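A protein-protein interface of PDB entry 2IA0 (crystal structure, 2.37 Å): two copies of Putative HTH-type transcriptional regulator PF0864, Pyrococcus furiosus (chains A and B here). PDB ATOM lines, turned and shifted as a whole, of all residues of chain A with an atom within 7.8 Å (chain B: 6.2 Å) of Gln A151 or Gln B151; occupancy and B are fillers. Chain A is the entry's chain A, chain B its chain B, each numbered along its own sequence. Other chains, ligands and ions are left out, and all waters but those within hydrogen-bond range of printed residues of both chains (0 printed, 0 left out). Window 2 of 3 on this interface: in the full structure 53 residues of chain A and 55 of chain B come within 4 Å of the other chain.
O of Leu B79 sits at hydrogen-bond distance from N of Phe B153 (2.7 Å). The backbone NH of Leu A79 sits at hydrogen-bond distance from the backbone carbonyl oxygen of Phe A153 (2.7 Å). The backbone NH (N) of Val A81 sits at hydrogen-bond distance from the backbone carbonyl oxygen (O) of Gln A151 (2.8 Å). The backbone NH (N) of Gln B151 sits at hydrogen-bond distance from the backbone carbonyl oxygen (O) of Val B81 (2.8 Å).
Hydrophobic or aromatic side chains of chain A that line the printed part of chain B: Leu A79, Val A81 and Phe A153. Printed residues of chain B that touch a printed residue of chain A: Leu B79, Val B81, Gln B151 and Phe B153. Among the printed residues, 5 pairs touch across the chains. Among the printed residues, no Asp or Glu carboxylate lies within 4 Å of a Lys or Arg side-chain nitrogen of the other chain.
Leu B79 touches Leu A79. CE1 of Phe B153 touches CG1 of Val A81 (3.7 Å). Lys A120 touches Phe B153 (CD to CE1, 3.7 Å). Val B81 touches Phe A153.
The side-chain amide nitrogen of Gln B151 lies within hydrogen-bond range of the side-chain amide oxygen of Gln A151 (2.9 Å).
Leu A79 touches its own counterpart, Leu B79. Val A81 touches Phe B153, and with the chains exchanged Phe A153 touches Val B81. Gln B151 touches its own counterpart, Gln A151. 9 positions are printed for both chains. Of the 5 pairs that touch across the chains among the printed residues, 4 have their exchanged pair printed and touching as well.
Ile A80 touches none of the printed residues of chain B. Of the printed residues of chain B, Lys A120 touches Phe B153. Gln A151 touches just one residue of chain B: Gln B151 (2.9 Å). Printed residues of chain B within 4 Å of Phe A153: Val B81. Of the printed residues of chain A, Leu B79 touches Leu A79 (3.7 Å). Of chain A, only Gln A151 (2.9 Å) comes within 4 Å of Gln B151. Ile B152 touches none of the printed residues of chain A. Of the printed residues of chain A, Phe B153 touches Val A81 (3.7 Å) and Lys A120 (3.7 Å). The nearest residue of chain B that does not touch Gln A151 is Phe B153 (4.1 Å). The nearest residue of chain A that does not touch Gln B151 is Phe A153 (4.05 Å). The nearest printed residue of chain A that does not touch Leu B79 is Val A81 (5.1 Å).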
ATOM      1  N   ALA A  78     -19.494 -29.196  16.792  1.00  0.00           N
ATOM      2  CA  ALA A  78     -20.473 -28.115  16.653  1.00  0.00           C
ATOM      3  C   ALA A  78     -21.484 -28.203  17.782  1.00  0.00           C
ATOM      4  O   ALA A  78     -21.855 -29.301  18.237  1.00  0.00           O
ATOM      5  CB  ALA A  78     -21.172 -28.172  15.311  1.00  0.00           C
ATOM      6  N   LEU A  79     -21.880 -27.045  18.282  1.00  0.00           N
ATOM      7  CA  LEU A  79     -22.978 -26.973  19.217  1.00  0.00           C
ATOM      8  C   LEU A  79     -24.251 -26.601  18.429  1.00  0.00           C
ATOM      9  O   LEU A  79     -24.229 -25.753  17.551  1.00  0.00           O
ATOM     10  CB  LEU A  79     -22.654 -25.945  20.292  1.00  0.00           C
ATOM     11  CG  LEU A  79     -23.790 -25.419  21.158  1.00  0.00           C
ATOM     12  CD1 LEU A  79     -24.125 -26.474  22.237  1.00  0.00           C
ATOM     13  CD2 LEU A  79     -23.348 -24.102  21.772  1.00  0.00           C
ATOM     14  N   ILE A  80     -25.353 -27.273  18.731  1.00  0.00           N
ATOM     15  CA  ILE A  80     -26.619 -27.084  18.008  1.00  0.00           C
ATOM     16  C   ILE A  80     -27.696 -26.650  18.980  1.00  0.00           C
ATOM     17  O   ILE A  80     -27.855 -27.254  20.020  1.00  0.00           O
ATOM     18  CB  ILE A  80     -27.046 -28.400  17.333  1.00  0.00           C
ATOM     19  CG1 ILE A  80     -25.878 -28.934  16.488  1.00  0.00           C
ATOM     20  CG2 ILE A  80     -28.330 -28.197  16.486  1.00  0.00           C
ATOM     21  CD1 ILE A  80     -26.207 -30.123  15.697  1.00  0.00           C
ATOM     22  N   VAL A  81     -28.413 -25.583  18.655  1.00  0.00           N
ATOM     23  CA  VAL A  81     -29.537 -25.152  19.490  1.00  0.00           C
ATOM     24  C   VAL A  81     -30.841 -25.138  18.703  1.00  0.00           C
ATOM     25  O   VAL A  81     -31.001 -24.388  17.747  1.00  0.00           O
ATOM     26  CB  VAL A  81     -29.288 -23.798  20.181  1.00  0.00           C
ATOM     27  CG1 VAL A  81     -30.417 -23.508  21.218  1.00  0.00           C
ATOM     28  CG2 VAL A  81     -27.909 -23.798  20.861  1.00  0.00           C
ATOM     29  N   LEU A  82     -31.755 -26.009  19.121  1.00  0.00           N
ATOM     30  CA  LEU A  82     -33.059 -26.184  18.505  1.00  0.00           C
ATOM     31  C   LEU A  82     -34.123 -25.558  19.393  1.00  0.00           C
ATOM     32  O   LEU A  82     -34.113 -25.756  20.598  1.00  0.00           O
ATOM     33  CB  LEU A  82     -33.370 -27.687  18.380  1.00  0.00           C
ATOM     34  CG  LEU A  82     -32.387 -28.578  17.633  1.00  0.00           C
ATOM     35  CD1 LEU A  82     -32.963 -29.967  17.529  1.00  0.00           C
ATOM     36  CD2 LEU A  82     -32.101 -28.015  16.257  1.00  0.00           C
ATOM     37  N   GLU A  83     -35.059 -24.835  18.800  1.00  0.00           N
ATOM     38  CA  GLU A  83     -36.200 -24.319  19.549  1.00  0.00           C
ATOM     39  C   GLU A  83     -37.479 -24.852  18.911  1.00  0.00           C
ATOM     40  O   GLU A  83     -37.710 -24.660  17.719  1.00  0.00           O
ATOM     41  CB  GLU A  83     -36.197 -22.784  19.549  1.00  0.00           C
ATOM     42  CG  GLU A  83     -37.378 -22.138  20.278  1.00  0.00           C
ATOM     43  CD  GLU A  83     -37.418 -20.624  20.103  1.00  0.00           C
ATOM     44  OE1 GLU A  83     -36.781 -20.098  19.161  1.00  0.00           O
ATOM     45  OE2 GLU A  83     -38.101 -19.945  20.899  1.00  0.00           O
ATOM     46  N   LYS A 120     -36.315 -25.827  24.206  1.00  0.00           N
ATOM     47  CA  LYS A 120     -35.028 -25.982  23.457  1.00  0.00           C
ATOM     48  C   LYS A 120     -34.227 -27.268  23.702  1.00  0.00           C
ATOM     49  O   LYS A 120     -34.239 -27.833  24.790  1.00  0.00           O
ATOM     50  CB  LYS A 120     -34.111 -24.779  23.691  1.00  0.00           C
ATOM     51  CG  LYS A 120     -34.792 -23.461  23.493  1.00  0.00           C
ATOM     52  CD  LYS A 120     -33.815 -22.313  23.353  1.00  0.00           C
ATOM     53  CE  LYS A 120     -34.570 -21.001  23.517  1.00  0.00           C
ATOM     54  NZ  LYS A 120     -35.526 -21.196  24.649  1.00  0.00           N
ATOM     55  N   ILE A 121     -33.513 -27.712  22.672  1.00  0.00           N
ATOM     56  CA  ILE A 121     -32.602 -28.856  22.791  1.00  0.00           C
ATOM     57  C   ILE A 121     -31.239 -28.370  22.385  1.00  0.00           C
ATOM     58  O   ILE A 121     -31.092 -27.707  21.369  1.00  0.00           O
ATOM     59  CB  ILE A 121     -32.982 -30.059  21.911  1.00  0.00           C
ATOM     60  CG1 ILE A 121     -34.366 -30.574  22.268  1.00  0.00           C
ATOM     61  CG2 ILE A 121     -31.980 -31.216  22.050  1.00  0.00           C
ATOM     62  CD1 ILE A 121     -35.329 -30.450  21.101  1.00  0.00           C
ATOM     63  N   ALA A 123     -27.371 -29.733  21.681  1.00  0.00           N
ATOM     64  CA  ALA A 123     -26.572 -30.915  21.346  1.00  0.00           C
ATOM     65  C   ALA A 123     -25.135 -30.580  20.975  1.00  0.00           C
ATOM     66  O   ALA A 123     -24.870 -29.557  20.368  1.00  0.00           O
ATOM     67  CB  ALA A 123     -27.213 -31.734  20.225  1.00  0.00           C
ATOM     68  N   ILE A 137     -26.507 -32.488   9.680  1.00  0.00           N
ATOM     69  CA  ILE A 137     -27.602 -31.522   9.818  1.00  0.00           C
ATOM     70  C   ILE A 137     -28.702 -31.680   8.749  1.00  0.00           C
ATOM     71  O   ILE A 137     -29.893 -31.645   9.093  1.00  0.00           O
ATOM     72  CB  ILE A 137     -27.058 -30.070   9.963  1.00  0.00           C
ATOM     73  CG1 ILE A 137     -26.335 -29.941  11.324  1.00  0.00           C
ATOM     74  CG2 ILE A 137     -28.182 -29.016   9.824  1.00  0.00           C
ATOM     75  CD1 ILE A 137     -25.188 -28.992  11.315  1.00  0.00           C
ATOM     76  N   ILE A 141     -31.386 -32.977  11.484  1.00  0.00           N
ATOM     77  CA  ILE A 141     -31.802 -31.720  12.130  1.00  0.00           C
ATOM     78  C   ILE A 141     -32.840 -30.913  11.328  1.00  0.00           C
ATOM     79  O   ILE A 141     -33.875 -30.529  11.861  1.00  0.00           O
ATOM     80  CB  ILE A 141     -30.566 -30.850  12.553  1.00  0.00           C
ATOM     81  CG1 ILE A 141     -29.651 -31.608  13.559  1.00  0.00           C
ATOM     82  CG2 ILE A 141     -30.982 -29.449  13.047  1.00  0.00           C
ATOM     83  CD1 ILE A 141     -30.287 -32.041  14.899  1.00  0.00           C
ATOM     84  N   HIS A 149     -36.577 -22.438  15.409  1.00  0.00           N
ATOM     85  CA  HIS A 149     -35.231 -21.970  15.156  1.00  0.00           C
ATOM     86  C   HIS A 149     -34.189 -23.078  15.253  1.00  0.00           C
ATOM     87  O   HIS A 149     -34.328 -23.991  16.044  1.00  0.00           O
ATOM     88  CB  HIS A 149     -34.879 -20.810  16.104  1.00  0.00           C
ATOM     89  CG  HIS A 149     -35.543 -19.517  15.742  1.00  0.00           C
ATOM     90  ND1 HIS A 149     -36.139 -18.693  16.677  1.00  0.00           N
ATOM     91  CD2 HIS A 149     -35.707 -18.903  14.542  1.00  0.00           C
ATOM     92  CE1 HIS A 149     -36.627 -17.625  16.069  1.00  0.00           C
ATOM     93  NE2 HIS A 149     -36.386 -17.733  14.773  1.00  0.00           N
ATOM     94  N   ILE A 150     -33.159 -22.984  14.417  1.00  0.00           N
ATOM     95  CA  ILE A 150     -31.989 -23.833  14.483  1.00  0.00           C
ATOM     96  C   ILE A 150     -30.756 -22.930  14.458  1.00  0.00           C
ATOM     97  O   ILE A 150     -30.621 -22.081  13.574  1.00  0.00           O
ATOM     98  CB  ILE A 150     -31.870 -24.800  13.277  1.00  0.00           C
ATOM     99  CG1 ILE A 150     -33.094 -25.708  13.139  1.00  0.00           C
ATOM    100  CG2 ILE A 150     -30.527 -25.612  13.343  1.00  0.00           C
ATOM    101  CD1 ILE A 150     -33.268 -26.242  11.705  1.00  0.00           C
ATOM    102  N   GLN A 151     -29.866 -23.108  15.430  1.00  0.00           N
ATOM    103  CA  GLN A 151     -28.574 -22.429  15.413  1.00  0.00           C
ATOM    104  C   GLN A 151     -27.437 -23.431  15.475  1.00  0.00           C
ATOM    105  O   GLN A 151     -27.511 -24.421  16.220  1.00  0.00           O
ATOM    106  CB  GLN A 151     -28.450 -21.432  16.553  1.00  0.00           C
ATOM    107  CG  GLN A 151     -29.579 -20.430  16.619  1.00  0.00           C
ATOM    108  CD  GLN A 151     -29.357 -19.433  17.700  1.00  0.00           C
ATOM    109  OE1 GLN A 151     -28.569 -18.518  17.546  1.00  0.00           O
ATOM    110  NE2 GLN A 151     -30.038 -19.608  18.819  1.00  0.00           N
ATOM    111  N   ILE A 152     -26.413 -23.190  14.653  1.00  0.00           N
ATOM    112  CA  ILE A 152     -25.223 -24.037  14.645  1.00  0.00           C
ATOM    113  C   ILE A 152     -23.972 -23.215  14.928  1.00  0.00           C
ATOM    114  O   ILE A 152     -23.669 -22.255  14.200  1.00  0.00           O
ATOM    115  CB  ILE A 152     -25.086 -24.907  13.353  1.00  0.00           C
ATOM    116  CG1 ILE A 152     -26.257 -25.894  13.269  1.00  0.00           C
ATOM    117  CG2 ILE A 152     -23.780 -25.712  13.373  1.00  0.00           C
ATOM    118  CD1 ILE A 152     -26.687 -26.144  11.876  1.00  0.00           C
ATOM    119  N   PHE A 153     -23.288 -23.592  16.019  1.00  0.00           N
ATOM    120  CA  PHE A 153     -22.066 -22.941  16.456  1.00  0.00           C
ATOM    121  C   PHE A 153     -20.940 -23.941  16.387  1.00  0.00           C
ATOM    122  O   PHE A 153     -20.801 -24.770  17.275  1.00  0.00           O
ATOM    123  CB  PHE A 153     -22.208 -22.406  17.882  1.00  0.00           C
ATOM    124  CG  PHE A 153     -23.394 -21.523  18.068  1.00  0.00           C
ATOM    125  CD1 PHE A 153     -23.387 -20.208  17.575  1.00  0.00           C
ATOM    126  CD2 PHE A 153     -24.532 -22.000  18.708  1.00  0.00           C
ATOM    127  CE1 PHE A 153     -24.503 -19.383  17.724  1.00  0.00           C
ATOM    128  CE2 PHE A 153     -25.652 -21.187  18.861  1.00  0.00           C
ATOM    129  CZ  PHE A 153     -25.638 -19.871  18.357  1.00  0.00           C
ATOM    130  N   PRO A 154     -20.139 -23.881  15.308  1.00  0.00           N
ATOM    131  CA  PRO A 154     -18.888 -24.657  15.169  1.00  0.00           C
ATOM    132  C   PRO A 154     -17.900 -24.301  16.292  1.00  0.00           C
ATOM    133  O   PRO A 154     -17.758 -23.126  16.626  1.00  0.00           O
ATOM    134  CB  PRO A 154     -18.308 -24.175  13.853  1.00  0.00           C
ATOM    135  CG  PRO A 154     -19.425 -23.436  13.136  1.00  0.00           C
ATOM    136  CD  PRO A 154     -20.414 -23.001  14.157  1.00  0.00           C
ATOM    137  N   LEU B  79     -25.666 -22.500  29.602  1.00  0.00           N
ATOM    138  CA  LEU B  79     -24.816 -22.309  28.456  1.00  0.00           C
ATOM    139  C   LEU B  79     -25.028 -20.910  27.847  1.00  0.00           C
ATOM    140  O   LEU B  79     -26.140 -20.461  27.668  1.00  0.00           O
ATOM    141  CB  LEU B  79     -25.007 -23.425  27.446  1.00  0.00           C
ATOM    142  CG  LEU B  79     -24.130 -23.426  26.205  1.00  0.00           C
ATOM    143  CD1 LEU B  79     -22.829 -24.198  26.421  1.00  0.00           C
ATOM    144  CD2 LEU B  79     -24.953 -24.008  25.056  1.00  0.00           C
ATOM    145  N   ILE B  80     -23.924 -20.234  27.556  1.00  0.00           N
ATOM    146  CA  ILE B  80     -23.923 -18.850  27.109  1.00  0.00           C
ATOM    147  C   ILE B  80     -23.177 -18.740  25.797  1.00  0.00           C
ATOM    148  O   ILE B  80     -22.069 -19.264  25.629  1.00  0.00           O
ATOM    149  CB  ILE B  80     -23.262 -17.951  28.152  1.00  0.00           C
ATOM    150  CG1 ILE B  80     -24.080 -17.973  29.459  1.00  0.00           C
ATOM    151  CG2 ILE B  80     -23.023 -16.548  27.598  1.00  0.00           C
ATOM    152  CD1 ILE B  80     -23.238 -17.689  30.675  1.00  0.00           C
ATOM    153  N   VAL B  81     -23.825 -18.084  24.853  1.00  0.00           N
ATOM    154  CA  VAL B  81     -23.234 -17.795  23.577  1.00  0.00           C
ATOM    155  C   VAL B  81     -23.230 -16.285  23.440  1.00  0.00           C
ATOM    156  O   VAL B  81     -24.261 -15.613  23.575  1.00  0.00           O
ATOM    157  CB  VAL B  81     -24.001 -18.436  22.424  1.00  0.00           C
ATOM    158  CG1 VAL B  81     -23.287 -18.152  21.096  1.00  0.00           C
ATOM    159  CG2 VAL B  81     -24.128 -19.908  22.642  1.00  0.00           C
ATOM    160  N   LEU B  82     -22.052 -15.764  23.164  1.00  0.00           N
ATOM    161  CA  LEU B  82     -21.815 -14.330  23.193  1.00  0.00           C
ATOM    162  C   LEU B  82     -21.227 -13.939  21.836  1.00  0.00           C
ATOM    163  O   LEU B  82     -20.454 -14.682  21.272  1.00  0.00           O
ATOM    164  CB  LEU B  82     -20.930 -14.065  24.412  1.00  0.00           C
ATOM    165  CG  LEU B  82     -19.783 -13.162  24.777  1.00  0.00           C
ATOM    166  CD1 LEU B  82     -19.277 -13.726  26.085  1.00  0.00           C
ATOM    167  CD2 LEU B  82     -18.688 -13.178  23.702  1.00  0.00           C
ATOM    168  N   HIS B 149     -24.447  -9.370  20.888  1.00  0.00           N
ATOM    169  CA  HIS B 149     -25.497 -10.320  21.263  1.00  0.00           C
ATOM    170  C   HIS B 149     -25.009 -11.255  22.365  1.00  0.00           C
ATOM    171  O   HIS B 149     -23.828 -11.602  22.419  1.00  0.00           O
ATOM    172  CB  HIS B 149     -25.943 -11.180  20.065  1.00  0.00           C
ATOM    173  CG  HIS B 149     -26.517 -10.412  18.911  1.00  0.00           C
ATOM    174  ND1 HIS B 149     -26.141 -10.650  17.603  1.00  0.00           N
ATOM    175  CD2 HIS B 149     -27.466  -9.446  18.854  1.00  0.00           C
ATOM    176  CE1 HIS B 149     -26.818  -9.854  16.793  1.00  0.00           C
ATOM    177  NE2 HIS B 149     -27.629  -9.109  17.528  1.00  0.00           N
ATOM    178  N   ILE B 150     -25.933 -11.656  23.239  1.00  0.00           N
ATOM    179  CA  ILE B 150     -25.733 -12.752  24.176  1.00  0.00           C
ATOM    180  C   ILE B 150     -27.019 -13.600  24.303  1.00  0.00           C
ATOM    181  O   ILE B 150     -28.115 -13.060  24.482  1.00  0.00           O
ATOM    182  CB  ILE B 150     -25.328 -12.302  25.594  1.00  0.00           C
ATOM    183  CG1 ILE B 150     -26.473 -11.567  26.285  1.00  0.00           C
ATOM    184  CG2 ILE B 150     -24.061 -11.451  25.604  1.00  0.00           C
ATOM    185  CD1 ILE B 150     -26.562 -11.893  27.758  1.00  0.00           C
ATOM    186  N   GLN B 151     -26.865 -14.921  24.205  1.00  0.00           N
ATOM    187  CA  GLN B 151     -27.935 -15.864  24.459  1.00  0.00           C
ATOM    188  C   GLN B 151     -27.559 -16.697  25.667  1.00  0.00           C
ATOM    189  O   GLN B 151     -26.441 -17.158  25.787  1.00  0.00           O
ATOM    190  CB  GLN B 151     -28.157 -16.756  23.258  1.00  0.00           C
ATOM    191  CG  GLN B 151     -28.443 -15.950  21.988  1.00  0.00           C
ATOM    192  CD  GLN B 151     -28.820 -16.821  20.824  1.00  0.00           C
ATOM    193  OE1 GLN B 151     -29.869 -17.444  20.840  1.00  0.00           O
ATOM    194  NE2 GLN B 151     -27.952 -16.886  19.810  1.00  0.00           N
ATOM    195  N   ILE B 152     -28.503 -16.840  26.578  1.00  0.00           N
ATOM    196  CA  ILE B 152     -28.329 -17.649  27.765  1.00  0.00           C
ATOM    197  C   ILE B 152     -29.312 -18.795  27.709  1.00  0.00           C
ATOM    198  O   ILE B 152     -30.508 -18.596  27.436  1.00  0.00           O
ATOM    199  CB  ILE B 152     -28.530 -16.813  29.030  1.00  0.00           C
ATOM    200  CG1 ILE B 152     -27.488 -15.689  29.026  1.00  0.00           C
ATOM    201  CG2 ILE B 152     -28.437 -17.696  30.272  1.00  0.00           C
ATOM    202  CD1 ILE B 152     -27.895 -14.499  29.741  1.00  0.00           C
ATOM    203  N   PHE B 153     -28.773 -19.998  27.901  1.00  0.00           N
ATOM    204  CA  PHE B 153     -29.543 -21.239  27.854  1.00  0.00           C
ATOM    205  C   PHE B 153     -29.352 -21.981  29.154  1.00  0.00           C
ATOM    206  O   PHE B 153     -28.417 -22.777  29.282  1.00  0.00           O
ATOM    207  CB  PHE B 153     -29.121 -22.130  26.670  1.00  0.00           C
ATOM    208  CG  PHE B 153     -29.224 -21.456  25.320  1.00  0.00           C
ATOM    209  CD1 PHE B 153     -30.458 -21.197  24.751  1.00  0.00           C
ATOM    210  CD2 PHE B 153     -28.074 -21.084  24.625  1.00  0.00           C
ATOM    211  CE1 PHE B 153     -30.550 -20.568  23.495  1.00  0.00           C
ATOM    212  CE2 PHE B 153     -28.153 -20.468  23.371  1.00  0.00           C
ATOM    213  CZ  PHE B 153     -29.391 -20.204  22.811  1.00  0.00           C
